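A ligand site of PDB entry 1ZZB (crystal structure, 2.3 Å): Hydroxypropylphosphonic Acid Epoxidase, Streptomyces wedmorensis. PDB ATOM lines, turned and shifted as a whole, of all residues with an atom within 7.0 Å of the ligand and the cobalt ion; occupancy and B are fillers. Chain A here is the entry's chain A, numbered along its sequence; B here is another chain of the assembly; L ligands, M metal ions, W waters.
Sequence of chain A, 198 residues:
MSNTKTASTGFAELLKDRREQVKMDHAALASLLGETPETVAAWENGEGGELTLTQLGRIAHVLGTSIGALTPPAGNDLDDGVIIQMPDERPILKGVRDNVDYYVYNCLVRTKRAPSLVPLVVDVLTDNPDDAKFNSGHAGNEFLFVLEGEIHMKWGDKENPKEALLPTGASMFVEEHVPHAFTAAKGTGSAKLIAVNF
The side-chain amino group (NZ) of Lys 23 of chain B lies within salt-bridge range of an oxygen (O2) of the ligand (2.8 Å). The side-chain hydroxyl (OH) of Tyr 105 lies close to an oxygen (O2) of the ligand (3.5 Å). ND2 of Asn 135 lies close to O3 of the ligand (3.3 Å).
OD1 of Asn 197 sits close to OE2 of Glu 142 (3.2 Å). The backbone NH (N) of Val 174 sits at hydrogen-bond distance from the backbone carbonyl oxygen (O) of Glu 142 (3.0 Å). O of His 180 lies within hydrogen-bond range of N of Asn 135, 3.1 Å away. A ring nitrogen (ND1) of His 180 lies within hydrogen-bond range of the backbone carbonyl oxygen (O) of Val 178, 2.8 Å away. The side-chain amide oxygen (OD1) of Asn 135 sits at hydrogen-bond distance from the backbone NH (N) of Gly 137 (2.5 Å). The side-chain hydroxyl (OH) of Tyr 103 is in hydrogen-bond range of the backbone NH (N) of Phe 182. The side-chain hydroxyl (OH) of Tyr 102 lies within hydrogen-bond range of the backbone NH (N) of Lys 133.
Merely in contact with the ligand: Tyr 103 and Lys 133. Eight residues have an atom within 4 Å of the ligand: Tyr 103, Tyr 105, Lys 133, Asn 135, His 138, Glu 142, His 180 and Lys 23 of chain B.
Asn 135 touches the cobalt ion (ND2 to CO, 3.99 Å). Of the 23 residues printed, 4 come within 4 Å of the cobalt ion.
The cobalt ion is bound by an oxygen (O3) of the ligand (1.9 Å), the side-chain carboxylate (OE2) of Glu 142 (2.1 Å), a ring nitrogen (NE2) of His 138 (2.1 Å), a ring nitrogen (NE2) of His 180 (2.3 Å) and water W1 (2.5 Å).
Water W1 bridges an oxygen (O4) of the ligand (2.6 Å) and the side-chain carboxylate of Glu 142 (2.9 Å).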
ATOM      1  N   TYR A 102      -7.283  32.915  20.305  1.00  0.00           N
ATOM      2  CA  TYR A 102      -7.207  31.535  19.830  1.00  0.00           C
ATOM      3  C   TYR A 102      -7.053  31.376  18.318  1.00  0.00           C
ATOM      4  O   TYR A 102      -6.210  30.598  17.860  1.00  0.00           O
ATOM      5  CB  TYR A 102      -8.441  30.775  20.299  1.00  0.00           C
ATOM      6  CG  TYR A 102      -8.256  29.273  20.425  1.00  0.00           C
ATOM      7  CD1 TYR A 102      -7.380  28.729  21.366  1.00  0.00           C
ATOM      8  CD2 TYR A 102      -8.982  28.401  19.614  1.00  0.00           C
ATOM      9  CE1 TYR A 102      -7.237  27.351  21.502  1.00  0.00           C
ATOM     10  CE2 TYR A 102      -8.838  27.013  19.748  1.00  0.00           C
ATOM     11  CZ  TYR A 102      -7.972  26.498  20.685  1.00  0.00           C
ATOM     12  OH  TYR A 102      -7.853  25.126  20.826  1.00  0.00           O
ATOM     13  N   TYR A 103      -7.887  32.084  17.549  1.00  0.00           N
ATOM     14  CA  TYR A 103      -7.838  32.020  16.089  1.00  0.00           C
ATOM     15  C   TYR A 103      -7.845  33.399  15.421  1.00  0.00           C
ATOM     16  O   TYR A 103      -8.054  34.441  16.047  1.00  0.00           O
ATOM     17  CB  TYR A 103      -9.075  31.300  15.528  1.00  0.00           C
ATOM     18  CG  TYR A 103      -9.283  29.848  15.903  1.00  0.00           C
ATOM     19  CD1 TYR A 103     -10.560  29.292  15.851  1.00  0.00           C
ATOM     20  CD2 TYR A 103      -8.225  29.028  16.293  1.00  0.00           C
ATOM     21  CE1 TYR A 103     -10.788  27.965  16.197  1.00  0.00           C
ATOM     22  CE2 TYR A 103      -8.450  27.682  16.636  1.00  0.00           C
ATOM     23  CZ  TYR A 103      -9.735  27.175  16.592  1.00  0.00           C
ATOM     24  OH  TYR A 103     -10.005  25.874  16.980  1.00  0.00           O
ATOM     25  N   TYR A 105      -9.644  34.497  11.844  1.00  0.00           N
ATOM     26  CA  TYR A 105     -10.453  34.077  10.707  1.00  0.00           C
ATOM     27  C   TYR A 105     -10.282  34.991   9.508  1.00  0.00           C
ATOM     28  O   TYR A 105     -10.524  36.200   9.592  1.00  0.00           O
ATOM     29  CB  TYR A 105     -11.929  34.053  11.071  1.00  0.00           C
ATOM     30  CG  TYR A 105     -12.273  33.191  12.258  1.00  0.00           C
ATOM     31  CD1 TYR A 105     -12.600  33.780  13.483  1.00  0.00           C
ATOM     32  CD2 TYR A 105     -12.299  31.801  12.158  1.00  0.00           C
ATOM     33  CE1 TYR A 105     -12.959  32.991  14.587  1.00  0.00           C
ATOM     34  CE2 TYR A 105     -12.654  31.006  13.247  1.00  0.00           C
ATOM     35  CZ  TYR A 105     -12.981  31.607  14.459  1.00  0.00           C
ATOM     36  OH  TYR A 105     -13.359  30.841  15.528  1.00  0.00           O
ATOM     37  N   LEU A 120     -13.395  29.564   5.291  1.00  0.00           N
ATOM     38  CA  LEU A 120     -12.400  30.374   5.975  1.00  0.00           C
ATOM     39  C   LEU A 120     -10.999  29.796   5.858  1.00  0.00           C
ATOM     40  O   LEU A 120     -10.808  28.619   5.531  1.00  0.00           O
ATOM     41  CB  LEU A 120     -12.726  30.443   7.469  1.00  0.00           C
ATOM     42  CG  LEU A 120     -14.163  30.681   7.914  1.00  0.00           C
ATOM     43  CD1 LEU A 120     -14.305  30.254   9.369  1.00  0.00           C
ATOM     44  CD2 LEU A 120     -14.533  32.157   7.744  1.00  0.00           C
ATOM     45  N   VAL A 122      -8.224  29.583   8.492  1.00  0.00           N
ATOM     46  CA  VAL A 122      -8.044  29.830   9.911  1.00  0.00           C
ATOM     47  C   VAL A 122      -6.602  29.681  10.355  1.00  0.00           C
ATOM     48  O   VAL A 122      -5.910  28.714   9.994  1.00  0.00           O
ATOM     49  CB  VAL A 122      -8.910  28.868  10.762  1.00  0.00           C
ATOM     50  CG1 VAL A 122      -8.818  29.244  12.235  1.00  0.00           C
ATOM     51  CG2 VAL A 122     -10.350  28.899  10.287  1.00  0.00           C
ATOM     52  N   LYS A 133      -9.456  24.994  23.705  1.00  0.00           N
ATOM     53  CA  LYS A 133     -10.777  25.428  24.151  1.00  0.00           C
ATOM     54  C   LYS A 133     -11.849  25.041  23.137  1.00  0.00           C
ATOM     55  O   LYS A 133     -11.964  25.645  22.061  1.00  0.00           O
ATOM     56  CB  LYS A 133     -10.788  26.944  24.380  1.00  0.00           C
ATOM     57  N   PHE A 134     -12.636  24.022  23.492  1.00  0.00           N
ATOM     58  CA  PHE A 134     -13.706  23.518  22.630  1.00  0.00           C
ATOM     59  C   PHE A 134     -14.786  24.551  22.411  1.00  0.00           C
ATOM     60  O   PHE A 134     -14.964  25.463  23.228  1.00  0.00           O
ATOM     61  CB  PHE A 134     -14.366  22.299  23.267  1.00  0.00           C
ATOM     62  CG  PHE A 134     -13.558  21.032  23.166  1.00  0.00           C
ATOM     63  CD1 PHE A 134     -12.302  20.945  23.766  1.00  0.00           C
ATOM     64  CD2 PHE A 134     -14.067  19.928  22.499  1.00  0.00           C
ATOM     65  CE1 PHE A 134     -11.580  19.747  23.716  1.00  0.00           C
ATOM     66  CE2 PHE A 134     -13.351  18.729  22.441  1.00  0.00           C
ATOM     67  CZ  PHE A 134     -12.098  18.640  23.054  1.00  0.00           C
ATOM     68  N   ASN A 135     -15.505  24.422  21.296  1.00  0.00           N
ATOM     69  CA  ASN A 135     -16.641  25.298  21.036  1.00  0.00           C
ATOM     70  C   ASN A 135     -17.784  24.410  21.510  1.00  0.00           C
ATOM     71  O   ASN A 135     -17.561  23.224  21.757  1.00  0.00           O
ATOM     72  CB  ASN A 135     -16.782  25.640  19.530  1.00  0.00           C
ATOM     73  CG  ASN A 135     -16.946  24.407  18.655  1.00  0.00           C
ATOM     74  OD1 ASN A 135     -17.695  23.489  19.001  1.00  0.00           O
ATOM     75  ND2 ASN A 135     -16.262  24.396  17.512  1.00  0.00           N
ATOM     76  N   SER A 136     -18.987  24.936  21.658  1.00  0.00           N
ATOM     77  CA  SER A 136     -20.097  24.115  22.137  1.00  0.00           C
ATOM     78  C   SER A 136     -20.715  23.285  21.009  1.00  0.00           C
ATOM     79  O   SER A 136     -21.732  22.613  21.197  1.00  0.00           O
ATOM     80  CB  SER A 136     -21.151  25.006  22.793  1.00  0.00           C
ATOM     81  N   GLY A 137     -20.069  23.312  19.845  1.00  0.00           N
ATOM     82  CA  GLY A 137     -20.590  22.597  18.691  1.00  0.00           C
ATOM     83  C   GLY A 137     -21.429  23.594  17.914  1.00  0.00           C
ATOM     84  O   GLY A 137     -22.007  24.510  18.510  1.00  0.00           O
ATOM     85  N   HIS A 138     -21.507  23.451  16.599  1.00  0.00           N
ATOM     86  CA  HIS A 138     -22.306  24.385  15.816  1.00  0.00           C
ATOM     87  C   HIS A 138     -23.077  23.701  14.691  1.00  0.00           C
ATOM     88  O   HIS A 138     -22.691  22.647  14.210  1.00  0.00           O
ATOM     89  CB  HIS A 138     -21.420  25.509  15.250  1.00  0.00           C
ATOM     90  CG  HIS A 138     -20.231  25.033  14.481  1.00  0.00           C
ATOM     91  ND1 HIS A 138     -20.339  24.315  13.309  1.00  0.00           N
ATOM     92  CD2 HIS A 138     -18.898  25.191  14.697  1.00  0.00           C
ATOM     93  CE1 HIS A 138     -19.125  24.051  12.835  1.00  0.00           C
ATOM     94  NE2 HIS A 138     -18.246  24.568  13.660  1.00  0.00           N
ATOM     95  N   GLU A 142     -18.808  20.539   8.588  1.00  0.00           N
ATOM     96  CA  GLU A 142     -17.594  21.289   8.339  1.00  0.00           C
ATOM     97  C   GLU A 142     -16.449  20.464   7.756  1.00  0.00           C
ATOM     98  O   GLU A 142     -15.984  19.508   8.368  1.00  0.00           O
ATOM     99  CB  GLU A 142     -17.124  21.972   9.624  1.00  0.00           C
ATOM    100  CG  GLU A 142     -15.879  22.838   9.456  1.00  0.00           C
ATOM    101  CD  GLU A 142     -15.552  23.657  10.700  1.00  0.00           C
ATOM    102  OE1 GLU A 142     -14.497  24.345  10.704  1.00  0.00           O
ATOM    103  OE2 GLU A 142     -16.341  23.626  11.670  1.00  0.00           O
ATOM    104  N   LEU A 144     -12.541  20.314   6.494  1.00  0.00           N
ATOM    105  CA  LEU A 144     -11.313  21.021   6.817  1.00  0.00           C
ATOM    106  C   LEU A 144     -10.145  20.427   6.057  1.00  0.00           C
ATOM    107  O   LEU A 144     -10.197  19.275   5.620  1.00  0.00           O
ATOM    108  CB  LEU A 144     -11.037  20.992   8.329  1.00  0.00           C
ATOM    109  CG  LEU A 144     -11.980  21.802   9.221  1.00  0.00           C
ATOM    110  CD1 LEU A 144     -13.177  20.961   9.601  1.00  0.00           C
ATOM    111  CD2 LEU A 144     -11.248  22.228  10.485  1.00  0.00           C
ATOM    112  N   VAL A 174     -16.274  17.181  10.236  1.00  0.00           N
ATOM    113  CA  VAL A 174     -16.907  17.070  11.546  1.00  0.00           C
ATOM    114  C   VAL A 174     -18.392  17.355  11.356  1.00  0.00           C
ATOM    115  O   VAL A 174     -18.794  18.399  10.838  1.00  0.00           O
ATOM    116  CB  VAL A 174     -16.245  18.010  12.623  1.00  0.00           C
ATOM    117  CG1 VAL A 174     -15.046  18.720  12.042  1.00  0.00           C
ATOM    118  CG2 VAL A 174     -17.263  18.973  13.197  1.00  0.00           C
ATOM    119  N   VAL A 178     -21.279  18.543  16.554  1.00  0.00           N
ATOM    120  CA  VAL A 178     -20.210  17.858  17.258  1.00  0.00           C
ATOM    121  C   VAL A 178     -19.199  18.904  17.722  1.00  0.00           C
ATOM    122  O   VAL A 178     -18.574  19.579  16.904  1.00  0.00           O
ATOM    123  CB  VAL A 178     -19.476  16.847  16.355  1.00  0.00           C
ATOM    124  CG1 VAL A 178     -18.279  16.282  17.098  1.00  0.00           C
ATOM    125  CG2 VAL A 178     -20.419  15.723  15.939  1.00  0.00           C
ATOM    126  N   HIS A 180     -15.827  20.720  18.883  1.00  0.00           N
ATOM    127  CA  HIS A 180     -14.432  20.500  18.530  1.00  0.00           C
ATOM    128  C   HIS A 180     -13.495  21.624  18.937  1.00  0.00           C
ATOM    129  O   HIS A 180     -13.931  22.705  19.321  1.00  0.00           O
ATOM    130  CB  HIS A 180     -14.296  20.266  17.014  1.00  0.00           C
ATOM    131  CG  HIS A 180     -15.075  21.232  16.182  1.00  0.00           C
ATOM    132  ND1 HIS A 180     -16.456  21.302  16.215  1.00  0.00           N
ATOM    133  CD2 HIS A 180     -14.669  22.159  15.282  1.00  0.00           C
ATOM    134  CE1 HIS A 180     -16.865  22.217  15.356  1.00  0.00           C
ATOM    135  NE2 HIS A 180     -15.807  22.746  14.780  1.00  0.00           N
ATOM    136  N   ALA A 181     -12.191  21.346  18.827  1.00  0.00           N
ATOM    137  CA  ALA A 181     -11.135  22.285  19.182  1.00  0.00           C
ATOM    138  C   ALA A 181      -9.874  21.998  18.346  1.00  0.00           C
ATOM    139  O   ALA A 181      -9.632  20.873  17.950  1.00  0.00           O
ATOM    140  CB  ALA A 181     -10.831  22.164  20.658  1.00  0.00           C
ATOM    141  N   PHE A 182      -9.070  23.031  18.113  1.00  0.00           N
ATOM    142  CA  PHE A 182      -7.854  22.882  17.326  1.00  0.00           C
ATOM    143  C   PHE A 182      -6.697  23.701  17.886  1.00  0.00           C
ATOM    144  O   PHE A 182      -6.904  24.776  18.439  1.00  0.00           O
ATOM    145  CB  PHE A 182      -8.101  23.348  15.886  1.00  0.00           C
ATOM    146  CG  PHE A 182      -9.053  22.479  15.109  1.00  0.00           C
ATOM    147  CD1 PHE A 182      -8.641  21.252  14.590  1.00  0.00           C
ATOM    148  CD2 PHE A 182     -10.370  22.892  14.893  1.00  0.00           C
ATOM    149  CE1 PHE A 182      -9.509  20.430  13.867  1.00  0.00           C
ATOM    150  CE2 PHE A 182     -11.262  22.076  14.175  1.00  0.00           C
ATOM    151  CZ  PHE A 182     -10.825  20.843  13.651  1.00  0.00           C
ATOM    152  N   ALA A 195     -11.140  25.889   6.499  1.00  0.00           N
ATOM    153  CA  ALA A 195     -12.338  25.267   7.046  1.00  0.00           C
ATOM    154  C   ALA A 195     -13.541  25.746   6.256  1.00  0.00           C
ATOM    155  O   ALA A 195     -13.667  26.939   5.955  1.00  0.00           O
ATOM    156  CB  ALA A 195     -12.484  25.632   8.513  1.00  0.00           C
ATOM    157  N   ASN A 197     -17.723  25.531   6.330  1.00  0.00           N
ATOM    158  CA  ASN A 197     -19.007  25.162   6.935  1.00  0.00           C
ATOM    159  C   ASN A 197     -20.028  25.175   5.805  1.00  0.00           C
ATOM    160  O   ASN A 197     -20.022  26.071   4.962  1.00  0.00           O
ATOM    161  CB  ASN A 197     -19.410  26.176   7.998  1.00  0.00           C
ATOM    162  CG  ASN A 197     -18.338  26.360   9.053  1.00  0.00           C
ATOM    163  OD1 ASN A 197     -18.262  25.612  10.027  1.00  0.00           O
ATOM    164  ND2 ASN A 197     -17.479  27.366   8.853  1.00  0.00           N
ATOM    165  N   GLU B  20     -22.384  34.232  15.100  1.00  0.00           N
ATOM    166  CA  GLU B  20     -21.294  33.346  15.489  1.00  0.00           C
ATOM    167  C   GLU B  20     -20.810  32.532  14.305  1.00  0.00           C
ATOM    168  O   GLU B  20     -19.598  32.385  14.117  1.00  0.00           O
ATOM    169  CB  GLU B  20     -21.740  32.429  16.648  1.00  0.00           C
ATOM    170  CG  GLU B  20     -21.857  33.173  17.976  1.00  0.00           C
ATOM    171  CD  GLU B  20     -22.294  32.287  19.142  1.00  0.00           C
ATOM    172  OE1 GLU B  20     -22.345  32.797  20.281  1.00  0.00           O
ATOM    173  OE2 GLU B  20     -22.588  31.096  18.919  1.00  0.00           O
ATOM    174  N   GLN B  21     -21.730  32.038  13.485  1.00  0.00           N
ATOM    175  CA  GLN B  21     -21.291  31.241  12.333  1.00  0.00           C
ATOM    176  C   GLN B  21     -20.574  32.050  11.250  1.00  0.00           C
ATOM    177  O   GLN B  21     -19.858  31.474  10.439  1.00  0.00           O
ATOM    178  CB  GLN B  21     -22.456  30.438  11.731  1.00  0.00           C
ATOM    179  CG  GLN B  21     -23.802  31.089  11.777  1.00  0.00           C
ATOM    180  CD  GLN B  21     -24.903  30.180  11.260  1.00  0.00           C
ATOM    181  OE1 GLN B  21     -24.844  29.702  10.128  1.00  0.00           O
ATOM    182  NE2 GLN B  21     -25.919  29.957  12.087  1.00  0.00           N
ATOM    183  N   LYS B  23     -18.498  34.324  12.135  1.00  0.00           N
ATOM    184  CA  LYS B  23     -17.341  34.756  12.910  1.00  0.00           C
ATOM    185  C   LYS B  23     -17.305  36.227  13.335  1.00  0.00           C
ATOM    186  O   LYS B  23     -16.221  36.774  13.594  1.00  0.00           O
ATOM    187  CB  LYS B  23     -16.057  34.421  12.141  1.00  0.00           C
ATOM    188  CG  LYS B  23     -16.035  33.001  11.605  1.00  0.00           C
ATOM    189  CD  LYS B  23     -16.426  31.986  12.672  1.00  0.00           C
ATOM    190  CE  LYS B  23     -16.703  30.615  12.065  1.00  0.00           C
ATOM    191  NZ  LYS B  23     -17.145  29.620  13.084  1.00  0.00           N
HETATM  192  P1  LIG L   1     -14.928  27.226  15.332  1.00  0.00           P
HETATM  193  C1  LIG L   1     -14.450  26.786  17.051  1.00  0.00           C
HETATM  194  C2  LIG L   1     -14.390  28.016  18.010  1.00  0.00           C
HETATM  195  O1  LIG L   1     -13.948  27.636  19.282  1.00  0.00           O
HETATM  196  C3  LIG L   1     -13.642  28.737  17.669  1.00  0.00           C
HETATM  197  O2  LIG L   1     -15.783  28.395  15.229  1.00  0.00           O
HETATM  198  O3  LIG L   1     -15.601  25.999  14.663  1.00  0.00           O
HETATM  199  O4  LIG L   1     -13.656  27.280  14.442  1.00  0.00           O
HETATM  200 CO    CO M   1     -16.117  24.601  13.527  1.00  0.00          CO
HETATM  201  O   HOH W   1     -13.614  24.926  13.414  1.00  0.00           O
